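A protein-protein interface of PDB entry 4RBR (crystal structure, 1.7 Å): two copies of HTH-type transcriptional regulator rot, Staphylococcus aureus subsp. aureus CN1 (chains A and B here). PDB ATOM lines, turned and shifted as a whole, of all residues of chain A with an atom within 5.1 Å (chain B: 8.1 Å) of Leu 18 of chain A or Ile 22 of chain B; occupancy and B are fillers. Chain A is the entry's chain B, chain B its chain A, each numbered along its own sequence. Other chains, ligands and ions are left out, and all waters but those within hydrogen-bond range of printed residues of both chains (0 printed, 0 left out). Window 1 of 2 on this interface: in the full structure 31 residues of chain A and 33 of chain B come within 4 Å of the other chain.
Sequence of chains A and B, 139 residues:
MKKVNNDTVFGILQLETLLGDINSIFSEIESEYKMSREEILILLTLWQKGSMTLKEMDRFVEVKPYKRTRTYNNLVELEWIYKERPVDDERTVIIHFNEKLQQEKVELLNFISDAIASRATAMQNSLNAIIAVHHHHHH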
ATOM      1  N   GLN A  14       8.726 -14.278  -7.977  1.00  0.00           N
ATOM      2  CA  GLN A  14       7.888 -13.217  -7.436  1.00  0.00           C
ATOM      3  C   GLN A  14       7.863 -13.210  -5.899  1.00  0.00           C
ATOM      4  O   GLN A  14       7.396 -12.236  -5.308  1.00  0.00           O
ATOM      5  CB  GLN A  14       6.469 -13.319  -7.982  1.00  0.00           C
ATOM      6  CG  GLN A  14       6.339 -12.868  -9.454  1.00  0.00           C
ATOM      7  CD  GLN A  14       6.481 -11.354  -9.619  1.00  0.00           C
ATOM      8  OE1 GLN A  14       5.692 -10.573  -9.078  1.00  0.00           O
ATOM      9  NE2 GLN A  14       7.478 -10.942 -10.371  1.00  0.00           N
ATOM     10  N   LEU A  15       8.330 -14.288  -5.255  1.00  0.00           N
ATOM     11  CA  LEU A  15       8.534 -14.234  -3.813  1.00  0.00           C
ATOM     12  C   LEU A  15       9.437 -13.049  -3.471  1.00  0.00           C
ATOM     13  O   LEU A  15       9.182 -12.313  -2.517  1.00  0.00           O
ATOM     14  CB  LEU A  15       9.149 -15.527  -3.280  1.00  0.00           C
ATOM     15  CG  LEU A  15       8.260 -16.764  -3.197  1.00  0.00           C
ATOM     16  CD1 LEU A  15       9.140 -17.975  -2.932  1.00  0.00           C
ATOM     17  CD2 LEU A  15       7.194 -16.602  -2.108  1.00  0.00           C
ATOM     18  N   GLU A  16      10.492 -12.872  -4.262  1.00  0.00           N
ATOM     19  CA  GLU A  16      11.460 -11.814  -4.007  1.00  0.00           C
ATOM     20  C   GLU A  16      10.837 -10.457  -4.293  1.00  0.00           C
ATOM     21  O   GLU A  16      11.124  -9.493  -3.600  1.00  0.00           O
ATOM     22  CB  GLU A  16      12.724 -12.029  -4.844  1.00  0.00           C
ATOM     23  CG  GLU A  16      13.942 -11.238  -4.382  1.00  0.00           C
ATOM     24  CD  GLU A  16      14.417 -11.632  -2.992  1.00  0.00           C
ATOM     25  OE1 GLU A  16      14.173 -12.773  -2.556  1.00  0.00           O
ATOM     26  OE2 GLU A  16      15.022 -10.784  -2.320  1.00  0.00           O
ATOM     27  N   THR A  17       9.982 -10.385  -5.316  1.00  0.00           N
ATOM     28  CA  THR A  17       9.278  -9.150  -5.645  1.00  0.00           C
ATOM     29  C   THR A  17       8.360  -8.700  -4.523  1.00  0.00           C
ATOM     30  O   THR A  17       8.299  -7.517  -4.185  1.00  0.00           O
ATOM     31  CB  THR A  17       8.431  -9.307  -6.940  1.00  0.00           C
ATOM     32  OG1 THR A  17       9.273  -9.792  -7.993  1.00  0.00           O
ATOM     33  CG2 THR A  17       7.809  -7.970  -7.340  1.00  0.00           C
ATOM     34  N   LEU A  18       7.645  -9.655  -3.944  1.00  0.00           N
ATOM     35  CA  LEU A  18       6.713  -9.358  -2.868  1.00  0.00           C
ATOM     36  C   LEU A  18       7.466  -8.927  -1.618  1.00  0.00           C
ATOM     37  O   LEU A  18       7.077  -7.972  -0.952  1.00  0.00           O
ATOM     38  CB  LEU A  18       5.836 -10.579  -2.574  1.00  0.00           C
ATOM     39  CG  LEU A  18       4.726 -10.388  -1.527  1.00  0.00           C
ATOM     40  CD1 LEU A  18       3.887  -9.141  -1.818  1.00  0.00           C
ATOM     41  CD2 LEU A  18       3.854 -11.626  -1.484  1.00  0.00           C
ATOM     42  N   LEU A  19       8.558  -9.626  -1.321  1.00  0.00           N
ATOM     43  CA  LEU A  19       9.426  -9.263  -0.200  1.00  0.00           C
ATOM     44  C   LEU A  19       9.910  -7.835  -0.371  1.00  0.00           C
ATOM     45  O   LEU A  19       9.934  -7.044   0.584  1.00  0.00           O
ATOM     46  CB  LEU A  19      10.615 -10.231  -0.099  1.00  0.00           C
ATOM     47  CG  LEU A  19      11.526 -10.153   1.127  1.00  0.00           C
ATOM     48  CD1 LEU A  19      11.449 -11.472   1.876  1.00  0.00           C
ATOM     49  CD2 LEU A  19      12.954  -9.875   0.732  1.00  0.00           C
ATOM     50  N   GLY A  20      10.300  -7.514  -1.596  1.00  0.00           N
ATOM     51  CA  GLY A  20      10.725  -6.170  -1.948  1.00  0.00           C
ATOM     52  C   GLY A  20       9.646  -5.135  -1.745  1.00  0.00           C
ATOM     53  O   GLY A  20       9.934  -4.024  -1.307  1.00  0.00           O
ATOM     54  N   ASP A  21       8.409  -5.478  -2.101  1.00  0.00           N
ATOM     55  CA  ASP A  21       7.272  -4.589  -1.857  1.00  0.00           C
ATOM     56  C   ASP A  21       7.164  -4.255  -0.372  1.00  0.00           C
ATOM     57  O   ASP A  21       6.981  -3.096   0.009  1.00  0.00           O
ATOM     58  CB  ASP A  21       5.956  -5.218  -2.312  1.00  0.00           C
ATOM     59  CG  ASP A  21       5.855  -5.380  -3.817  1.00  0.00           C
ATOM     60  OD1 ASP A  21       6.484  -4.600  -4.561  1.00  0.00           O
ATOM     61  OD2 ASP A  21       5.105  -6.279  -4.251  1.00  0.00           O
ATOM     62  N   ILE A  22       7.258  -5.289   0.457  1.00  0.00           N
ATOM     63  CA  ILE A  22       7.085  -5.134   1.893  1.00  0.00           C
ATOM     64  C   ILE A  22       8.224  -4.290   2.474  1.00  0.00           C
ATOM     65  O   ILE A  22       7.989  -3.339   3.221  1.00  0.00           O
ATOM     66  CB  ILE A  22       7.022  -6.502   2.602  1.00  0.00           C
ATOM     67  CG1 ILE A  22       5.741  -7.238   2.201  1.00  0.00           C
ATOM     68  CG2 ILE A  22       7.049  -6.316   4.109  1.00  0.00           C
ATOM     69  CD1 ILE A  22       5.716  -8.704   2.638  1.00  0.00           C
ATOM     70  N   MET A 123       1.051  -6.017  -5.078  1.00  0.00           N
ATOM     71  CA  MET A 123       1.308  -7.093  -4.115  1.00  0.00           C
ATOM     72  C   MET A 123       0.393  -8.293  -4.342  1.00  0.00           C
ATOM     73  O   MET A 123       0.843  -9.434  -4.299  1.00  0.00           O
ATOM     74  CB  MET A 123       1.171  -6.581  -2.683  1.00  0.00           C
ATOM     75  CG  MET A 123       2.325  -5.655  -2.290  1.00  0.00           C
ATOM     76  SD  MET A 123       2.340  -5.265  -0.540  1.00  0.00           S
ATOM     77  CE  MET A 123       0.758  -4.453  -0.391  1.00  0.00           C
ATOM     78  N   SER A 126       1.481 -10.109  -7.434  1.00  0.00           N
ATOM     79  CA  SER A 126       2.640 -10.938  -7.122  1.00  0.00           C
ATOM     80  C   SER A 126       2.255 -12.206  -6.371  1.00  0.00           C
ATOM     81  O   SER A 126       2.720 -13.301  -6.707  1.00  0.00           O
ATOM     82  CB  SER A 126       3.664 -10.152  -6.297  1.00  0.00           C
ATOM     83  OG  SER A 126       4.354  -9.216  -7.109  1.00  0.00           O
ATOM     84  N   LEU A 127       1.432 -12.055  -5.337  1.00  0.00           N
ATOM     85  CA  LEU A 127       1.011 -13.212  -4.567  1.00  0.00           C
ATOM     86  C   LEU A 127       0.204 -14.175  -5.446  1.00  0.00           C
ATOM     87  O   LEU A 127       0.323 -15.380  -5.279  1.00  0.00           O
ATOM     88  CB  LEU A 127       0.204 -12.818  -3.329  1.00  0.00           C
ATOM     89  CG  LEU A 127      -0.161 -14.015  -2.439  1.00  0.00           C
ATOM     90  CD1 LEU A 127       1.089 -14.750  -1.929  1.00  0.00           C
ATOM     91  CD2 LEU A 127      -1.048 -13.547  -1.279  1.00  0.00           C
ATOM     92  N   ILE A 130       2.824 -16.133  -7.310  1.00  0.00           N
ATOM     93  CA  ILE A 130       3.432 -17.069  -6.366  1.00  0.00           C
ATOM     94  C   ILE A 130       2.544 -18.285  -6.120  1.00  0.00           C
ATOM     95  O   ILE A 130       2.999 -19.427  -6.190  1.00  0.00           O
ATOM     96  CB  ILE A 130       3.724 -16.369  -5.010  1.00  0.00           C
ATOM     97  CG1 ILE A 130       4.755 -15.258  -5.210  1.00  0.00           C
ATOM     98  CG2 ILE A 130       4.164 -17.390  -3.950  1.00  0.00           C
ATOM     99  CD1 ILE A 130       4.782 -14.257  -4.091  1.00  0.00           C
ATOM    100  N   LEU B  15       2.335  -7.112   7.745  1.00  0.00           N
ATOM    101  CA  LEU B  15       3.413  -6.941   6.776  1.00  0.00           C
ATOM    102  C   LEU B  15       4.591  -7.813   7.178  1.00  0.00           C
ATOM    103  O   LEU B  15       5.196  -8.489   6.345  1.00  0.00           O
ATOM    104  CB  LEU B  15       3.845  -5.468   6.675  1.00  0.00           C
ATOM    105  CG  LEU B  15       2.939  -4.521   5.894  1.00  0.00           C
ATOM    106  CD1 LEU B  15       3.333  -3.070   6.181  1.00  0.00           C
ATOM    107  CD2 LEU B  15       2.993  -4.783   4.397  1.00  0.00           C
ATOM    108  N   GLU B  16       4.888  -7.806   8.473  1.00  0.00           N
ATOM    109  CA  GLU B  16       6.026  -8.521   9.008  1.00  0.00           C
ATOM    110  C   GLU B  16       5.718 -10.015   9.020  1.00  0.00           C
ATOM    111  O   GLU B  16       6.597 -10.845   8.830  1.00  0.00           O
ATOM    112  CB  GLU B  16       6.348  -8.017  10.417  1.00  0.00           C
ATOM    113  CG  GLU B  16       7.697  -8.432  10.956  1.00  0.00           C
ATOM    114  CD  GLU B  16       8.865  -7.778  10.234  1.00  0.00           C
ATOM    115  OE1 GLU B  16       8.673  -6.769   9.517  1.00  0.00           O
ATOM    116  OE2 GLU B  16       9.992  -8.284  10.382  1.00  0.00           O
ATOM    117  N   THR B  17       4.453 -10.351   9.232  1.00  0.00           N
ATOM    118  CA  THR B  17       4.044 -11.748   9.189  1.00  0.00           C
ATOM    119  C   THR B  17       4.229 -12.344   7.798  1.00  0.00           C
ATOM    120  O   THR B  17       4.726 -13.464   7.639  1.00  0.00           O
ATOM    121  CB  THR B  17       2.575 -11.913   9.607  1.00  0.00           C
ATOM    122  OG1 THR B  17       2.390 -11.352  10.914  1.00  0.00           O
ATOM    123  CG2 THR B  17       2.201 -13.380   9.622  1.00  0.00           C
ATOM    124  N   LEU B  18       3.809 -11.599   6.787  1.00  0.00           N
ATOM    125  CA  LEU B  18       3.911 -12.072   5.426  1.00  0.00           C
ATOM    126  C   LEU B  18       5.377 -12.172   5.036  1.00  0.00           C
ATOM    127  O   LEU B  18       5.805 -13.138   4.408  1.00  0.00           O
ATOM    128  CB  LEU B  18       3.150 -11.148   4.486  1.00  0.00           C
ATOM    129  CG  LEU B  18       3.182 -11.502   2.995  1.00  0.00           C
ATOM    130  CD1 LEU B  18       2.726 -12.955   2.763  1.00  0.00           C
ATOM    131  CD2 LEU B  18       2.327 -10.507   2.229  1.00  0.00           C
ATOM    132  N   LEU B  19       6.144 -11.168   5.440  1.00  0.00           N
ATOM    133  CA  LEU B  19       7.585 -11.186   5.269  1.00  0.00           C
ATOM    134  C   LEU B  19       8.188 -12.452   5.871  1.00  0.00           C
ATOM    135  O   LEU B  19       8.994 -13.144   5.234  1.00  0.00           O
ATOM    136  CB  LEU B  19       8.202  -9.946   5.921  1.00  0.00           C
ATOM    137  CG  LEU B  19       9.690  -9.764   5.688  1.00  0.00           C
ATOM    138  CD1 LEU B  19       9.874  -9.370   4.245  1.00  0.00           C
ATOM    139  CD2 LEU B  19      10.241  -8.696   6.625  1.00  0.00           C
ATOM    140  N   GLY B  20       7.802 -12.757   7.104  1.00  0.00           N
ATOM    141  CA  GLY B  20       8.269 -13.964   7.756  1.00  0.00           C
ATOM    142  C   GLY B  20       7.919 -15.224   6.980  1.00  0.00           C
ATOM    143  O   GLY B  20       8.716 -16.136   6.891  1.00  0.00           O
ATOM    144  N   ASP B  21       6.718 -15.261   6.408  1.00  0.00           N
ATOM    145  CA  ASP B  21       6.263 -16.397   5.615  1.00  0.00           C
ATOM    146  C   ASP B  21       7.196 -16.632   4.436  1.00  0.00           C
ATOM    147  O   ASP B  21       7.616 -17.758   4.155  1.00  0.00           O
ATOM    148  CB  ASP B  21       4.841 -16.159   5.097  1.00  0.00           C
ATOM    149  CG  ASP B  21       3.787 -16.195   6.187  1.00  0.00           C
ATOM    150  OD1 ASP B  21       4.061 -16.721   7.290  1.00  0.00           O
ATOM    151  OD2 ASP B  21       2.654 -15.727   5.921  1.00  0.00           O
ATOM    152  N   ILE B  22       7.528 -15.539   3.763  1.00  0.00           N
ATOM    153  CA  ILE B  22       8.345 -15.608   2.559  1.00  0.00           C
ATOM    154  C   ILE B  22       9.751 -16.065   2.927  1.00  0.00           C
ATOM    155  O   ILE B  22      10.287 -16.981   2.321  1.00  0.00           O
ATOM    156  CB  ILE B  22       8.370 -14.259   1.837  1.00  0.00           C
ATOM    157  CG1 ILE B  22       6.983 -13.975   1.240  1.00  0.00           C
ATOM    158  CG2 ILE B  22       9.415 -14.240   0.732  1.00  0.00           C
ATOM    159  CD1 ILE B  22       6.799 -12.540   0.801  1.00  0.00           C
ATOM    160  N   ASN B  23      10.330 -15.460   3.960  1.00  0.00           N
ATOM    161  CA  ASN B  23      11.671 -15.854   4.378  1.00  0.00           C
ATOM    162  C   ASN B  23      11.722 -17.284   4.907  1.00  0.00           C
ATOM    163  O   ASN B  23      12.728 -17.967   4.713  1.00  0.00           O
ATOM    164  CB  ASN B  23      12.199 -14.867   5.414  1.00  0.00           C
ATOM    165  CG  ASN B  23      12.625 -13.542   4.781  1.00  0.00           C
ATOM    166  OD1 ASN B  23      13.125 -13.523   3.656  1.00  0.00           O
ATOM    167  ND2 ASN B  23      12.421 -12.439   5.493  1.00  0.00           N
ATOM    168  N   SER B  24      10.644 -17.755   5.534  1.00  0.00           N
ATOM    169  CA  SER B  24      10.607 -19.138   6.003  1.00  0.00           C
ATOM    170  C   SER B  24      10.614 -20.123   4.836  1.00  0.00           C
ATOM    171  O   SER B  24      11.158 -21.212   4.958  1.00  0.00           O
ATOM    172  CB  SER B  24       9.388 -19.402   6.916  1.00  0.00           C
ATOM    173  OG  SER B  24       8.196 -19.687   6.201  1.00  0.00           O
ATOM    174  N   ILE B  25      10.004 -19.753   3.708  1.00  0.00           N
ATOM    175  CA  ILE B  25      10.117 -20.573   2.512  1.00  0.00           C
ATOM    176  C   ILE B  25      11.579 -20.681   2.094  1.00  0.00           C
ATOM    177  O   ILE B  25      12.104 -21.780   1.882  1.00  0.00           O
ATOM    178  CB  ILE B  25       9.262 -19.992   1.353  1.00  0.00           C
ATOM    179  CG1 ILE B  25       7.794 -20.013   1.767  1.00  0.00           C
ATOM    180  CG2 ILE B  25       9.499 -20.763   0.048  1.00  0.00           C
ATOM    181  CD1 ILE B  25       6.835 -19.289   0.822  1.00  0.00           C
ATOM    182  N   PHE B  26      12.244 -19.540   1.970  1.00  0.00           N
ATOM    183  CA  PHE B  26      13.652 -19.587   1.596  1.00  0.00           C
ATOM    184  C   PHE B  26      14.467 -20.383   2.626  1.00  0.00           C
ATOM    185  O   PHE B  26      15.278 -21.222   2.239  1.00  0.00           O
ATOM    186  CB  PHE B  26      14.201 -18.179   1.410  1.00  0.00           C
ATOM    187  CG  PHE B  26      13.780 -17.546   0.102  1.00  0.00           C
ATOM    188  CD1 PHE B  26      14.263 -18.041  -1.103  1.00  0.00           C
ATOM    189  CD2 PHE B  26      12.899 -16.479   0.076  1.00  0.00           C
ATOM    190  CE1 PHE B  26      13.879 -17.474  -2.325  1.00  0.00           C
ATOM    191  CE2 PHE B  26      12.507 -15.904  -1.140  1.00  0.00           C
ATOM    192  CZ  PHE B  26      13.001 -16.411  -2.342  1.00  0.00           C
ATOM    193  N   SER B  27      14.231 -20.161   3.920  1.00  0.00           N
ATOM    194  CA  SER B  27      14.939 -20.944   4.935  1.00  0.00           C
ATOM    195  C   SER B  27      14.759 -22.439   4.728  1.00  0.00           C
ATOM    196  O   SER B  27      15.709 -23.221   4.856  1.00  0.00           O
ATOM    197  CB  SER B  27      14.472 -20.559   6.346  1.00  0.00           C
ATOM    198  OG  SER B  27      14.832 -19.220   6.633  1.00  0.00           O
ATOM    199  N   GLU B  28      13.536 -22.845   4.399  1.00  0.00           N
ATOM    200  CA  GLU B  28      13.234 -24.258   4.230  1.00  0.00           C
ATOM    201  C   GLU B  28      14.010 -24.866   3.058  1.00  0.00           C
ATOM    202  O   GLU B  28      14.581 -25.951   3.173  1.00  0.00           O
ATOM    203  CB  GLU B  28      11.726 -24.453   4.030  1.00  0.00           C
ATOM    204  CG  GLU B  28      11.227 -25.881   4.266  1.00  0.00           C
ATOM    205  CD  GLU B  28       9.765 -26.052   3.851  1.00  0.00           C
ATOM    206  OE1 GLU B  28       9.040 -25.042   3.849  1.00  0.00           O
ATOM    207  OE2 GLU B  28       9.355 -27.193   3.522  1.00  0.00           O
ATOM    208  N   ILE B  29      14.038 -24.155   1.936  1.00  0.00           N
ATOM    209  CA  ILE B  29      14.816 -24.572   0.780  1.00  0.00           C
ATOM    210  C   ILE B  29      16.304 -24.607   1.094  1.00  0.00           C
ATOM    211  O   ILE B  29      17.017 -25.528   0.689  1.00  0.00           O
ATOM    212  CB  ILE B  29      14.595 -23.631  -0.399  1.00  0.00           C
ATOM    213  CG1 ILE B  29      13.107 -23.558  -0.737  1.00  0.00           C
ATOM    214  CG2 ILE B  29      15.412 -24.065  -1.612  1.00  0.00           C
ATOM    215  CD1 ILE B  29      12.749 -22.288  -1.510  1.00  0.00           C
ATOM    216  N   GLU B  30      16.760 -23.582   1.807  1.00  0.00           N
ATOM    217  CA  GLU B  30      18.174 -23.457   2.154  1.00  0.00           C
ATOM    218  C   GLU B  30      18.646 -24.650   2.977  1.00  0.00           C
ATOM    219  O   GLU B  30      19.713 -25.213   2.704  1.00  0.00           O
ATOM    220  CB  GLU B  30      18.422 -22.137   2.898  1.00  0.00           C
ATOM    221  CG  GLU B  30      18.420 -20.926   1.958  1.00  0.00           C
ATOM    222  CD  GLU B  30      18.100 -19.614   2.647  1.00  0.00           C
ATOM    223  OE1 GLU B  30      18.321 -19.496   3.865  1.00  0.00           O
ATOM    224  OE2 GLU B  30      17.605 -18.696   1.963  1.00  0.00           O
ATOM    225  N   ARG B  37      20.316 -18.153  -0.006  1.00  0.00           N
ATOM    226  CA  ARG B  37      19.229 -17.543  -0.757  1.00  0.00           C
ATOM    227  C   ARG B  37      19.722 -17.042  -2.106  1.00  0.00           C
ATOM    228  O   ARG B  37      19.032 -17.191  -3.113  1.00  0.00           O
ATOM    229  CB  ARG B  37      18.583 -16.385   0.003  1.00  0.00           C
ATOM    230  CG  ARG B  37      17.388 -15.830  -0.763  1.00  0.00           C
ATOM    231  CD  ARG B  37      16.661 -14.753  -0.011  1.00  0.00           C
ATOM    232  NE  ARG B  37      16.207 -15.238   1.284  1.00  0.00           N
ATOM    233  CZ  ARG B  37      15.374 -14.571   2.067  1.00  0.00           C
ATOM    234  NH1 ARG B  37      14.904 -13.391   1.678  1.00  0.00           N
ATOM    235  NH2 ARG B  37      15.020 -15.073   3.237  1.00  0.00           N
ATOM    236  N   ILE B 116       5.415 -23.344  -1.053  1.00  0.00           N
ATOM    237  CA  ILE B 116       4.426 -22.299  -1.327  1.00  0.00           C
ATOM    238  C   ILE B 116       2.990 -22.739  -1.053  1.00  0.00           C
ATOM    239  O   ILE B 116       2.215 -22.007  -0.439  1.00  0.00           O
ATOM    240  CB  ILE B 116       4.515 -21.831  -2.794  1.00  0.00           C
ATOM    241  CG1 ILE B 116       5.803 -21.047  -2.982  1.00  0.00           C
ATOM    242  CG2 ILE B 116       3.292 -20.958  -3.182  1.00  0.00           C
ATOM    243  CD1 ILE B 116       6.146 -20.781  -4.437  1.00  0.00           C
ATOM    244  N   ARG B 119       1.754 -22.741   2.473  1.00  0.00           N
ATOM    245  CA  ARG B 119       1.589 -21.412   3.058  1.00  0.00           C
ATOM    246  C   ARG B 119       0.579 -20.530   2.336  1.00  0.00           C
ATOM    247  O   ARG B 119       0.360 -19.396   2.763  1.00  0.00           O
ATOM    248  CB  ARG B 119       2.935 -20.682   3.088  1.00  0.00           C
ATOM    249  CG  ARG B 119       3.882 -21.141   4.179  1.00  0.00           C
ATOM    250  CD  ARG B 119       5.249 -21.242   3.607  1.00  0.00           C
ATOM    251  NE  ARG B 119       6.314 -21.440   4.588  1.00  0.00           N
ATOM    252  CZ  ARG B 119       7.111 -22.503   4.604  1.00  0.00           C
ATOM    253  NH1 ARG B 119       6.926 -23.464   3.711  1.00  0.00           N
ATOM    254  NH2 ARG B 119       8.088 -22.609   5.506  1.00  0.00           N
ATOM    255  N   MET B 123      -0.625 -16.871   3.659  1.00  0.00           N
ATOM    256  CA  MET B 123      -0.109 -15.673   2.997  1.00  0.00           C
ATOM    257  C   MET B 123      -1.232 -14.790   2.479  1.00  0.00           C
ATOM    258  O   MET B 123      -1.164 -13.573   2.573  1.00  0.00           O
ATOM    259  CB  MET B 123       0.827 -16.074   1.857  1.00  0.00           C
ATOM    260  CG  MET B 123       2.114 -16.695   2.393  1.00  0.00           C
ATOM    261  SD  MET B 123       3.415 -16.909   1.172  1.00  0.00           S
ATOM    262  CE  MET B 123       2.614 -17.892  -0.101  1.00  0.00           C
ATOM    263  N   GLN B 124      -2.269 -15.400   1.921  1.00  0.00           N
ATOM    264  CA  GLN B 124      -3.382 -14.618   1.391  1.00  0.00           C
ATOM    265  C   GLN B 124      -4.173 -13.992   2.533  1.00  0.00           C
ATOM    266  O   GLN B 124      -4.608 -12.855   2.434  1.00  0.00           O
ATOM    267  CB  GLN B 124      -4.302 -15.478   0.516  1.00  0.00           C
ATOM    268  CG  GLN B 124      -5.443 -14.682  -0.127  1.00  0.00           C
ATOM    269  CD  GLN B 124      -4.926 -13.667  -1.107  1.00  0.00           C
ATOM    270  OE1 GLN B 124      -4.293 -14.032  -2.104  1.00  0.00           O
ATOM    271  NE2 GLN B 124      -5.167 -12.376  -0.832  1.00  0.00           N
ATOM    272  N   LEU B 127      -2.105 -11.074   3.579  1.00  0.00           N
ATOM    273  CA  LEU B 127      -2.187  -9.978   2.613  1.00  0.00           C
ATOM    274  C   LEU B 127      -3.580  -9.340   2.650  1.00  0.00           C
ATOM    275  O   LEU B 127      -3.704  -8.131   2.458  1.00  0.00           O
ATOM    276  CB  LEU B 127      -1.848 -10.435   1.184  1.00  0.00           C
ATOM    277  CG  LEU B 127      -1.759  -9.297   0.162  1.00  0.00           C
ATOM    278  CD1 LEU B 127      -0.638  -8.333   0.568  1.00  0.00           C
ATOM    279  CD2 LEU B 127      -1.540  -9.812  -1.256  1.00  0.00           C
ATOM    280  N   ILE B 130      -3.408  -6.894   5.450  1.00  0.00           N
ATOM    281  CA  ILE B 130      -2.594  -5.752   5.044  1.00  0.00           C
ATOM    282  C   ILE B 130      -3.378  -4.771   4.177  1.00  0.00           C
ATOM    283  O   ILE B 130      -3.342  -3.567   4.406  1.00  0.00           O
ATOM    284  CB  ILE B 130      -1.347  -6.224   4.273  1.00  0.00           C
ATOM    285  CG1 ILE B 130      -0.395  -6.986   5.197  1.00  0.00           C
ATOM    286  CG2 ILE B 130      -0.646  -5.032   3.585  1.00  0.00           C
ATOM    287  CD1 ILE B 130       0.603  -7.846   4.438  1.00  0.00           C
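OG of Ser 27 of chain B lies within hydrogen-bond range of O of Asn 23 of chain B, 3.1 Å away. The side-chain amide oxygen (OD1) of Asn 23 of chain B lies within hydrogen-bond range of the guanidinium group (NH2) of Arg 37 of chain B, at 2.5 Å. The guanidinium group (NE) of Arg 37 of chain B is in salt-bridge range of the side-chain carboxylate (OE2) of Glu 30 of chain B (3.8 Å).
Among the printed residues, merely in contact across the chains: Leu 19 of chain A with Asn 23 of chain B (3.2 Å), Leu 127 of chain A with Gln 124 of chain B (3.4 Å), Ile 130 of chain A with Ile 116 of chain B (3.4 Å), Leu 19 of chain A with Leu 19 of chain B (3.5 Å), Leu 19 of chain A with Ile 22 of chain B (3.6 Å), Ile 22 of chain A with Leu 15 of chain B (3.6 Å), Ile 22 of chain A with Leu 19 of chain B (3.8 Å), Leu 127 of chain A with Leu 127 of chain B (3.8 Å), Leu 15 of chain A with Ile 22 of chain B (3.8 Å), Leu 18 of chain A with Ile 22 of chain B (3.8 Å), Ile 22 of chain A with Leu 18 of chain B (3.8 Å), Glu 16 of chain A with Phe 26 of chain B (3.8 Å), Leu 127 of chain A with Met 123 of chain B (3.9 Å), Met 123 of chain A with Leu 127 of chain B (3.9 Å), Leu 19 of chain A with Arg 37 of chain B (3.96 Å), Leu 15 of chain A with Ile 25 of chain B (3.99 Å) and Leu 15 of chain A with Phe 26 of chain B (3.9997 Å).
Of chain B, only Ile 22 (3.8 Å) comes within 4 Å of Leu 18 of chain A. Of chain A, only Leu 15 (3.8 Å), Leu 18 (3.8 Å) and Leu 19 (3.6 Å) come within 4 Å of Ile 22 of chain B. Printed residues of chain A within 4 Å of Leu 127 of chain B: Met 123 and Leu 127. Of the printed residues of chain A, Asn 23 of chain B touches Leu 19 (3.2 Å). Of the printed residues of chain B, Leu 15 of chain A touches Ile 22 (3.8 Å), Ile 25 (3.99 Å) and Phe 26 (3.9997 Å). Of the printed residues of chain B, Met 123 of chain A touches Leu 127. Printed residues of chain B within 4 Å of Ile 22 of chain A: Leu 15 (3.6 Å), Leu 18 (3.8 Å) and Leu 19 (3.8 Å). Ile 29 of chain B touches none of the printed residues of chain A. The nearest residue of chain B that does not touch Leu 18 of chain A is Leu 18 of chain B (4.2 Å).
Hydrophobic or aromatic side chains of chain A within 4 Å of the printed part of chain B: Leu 15, Leu 18, Leu 19, Ile 22, Leu 127 and Ile 130. Of the 23 printed residues of chain B, 12 touch a printed residue of chain A. Among the printed residues, 17 pairs touch across the chains.
Leu 15 of chain A touches Ile 22 of chain B, and with the chains exchanged Ile 22 of chain A touches Leu 15 of chain B. Leu 18 of chain A touches Ile 22 of chain B, and with the chains exchanged Ile 22 of chain A touches Leu 18 of chain B. Leu 19 of chain A touches Ile 22 of chain B, and with the chains exchanged Ile 22 of chain A touches Leu 19 of chain B. Leu 127 of chain B touches its own counterpart, Leu 127 of chain A. Positions printed for both chains: 15, 16, 17, 18, 19, 20, 21, 22, 123, 127 and 130.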
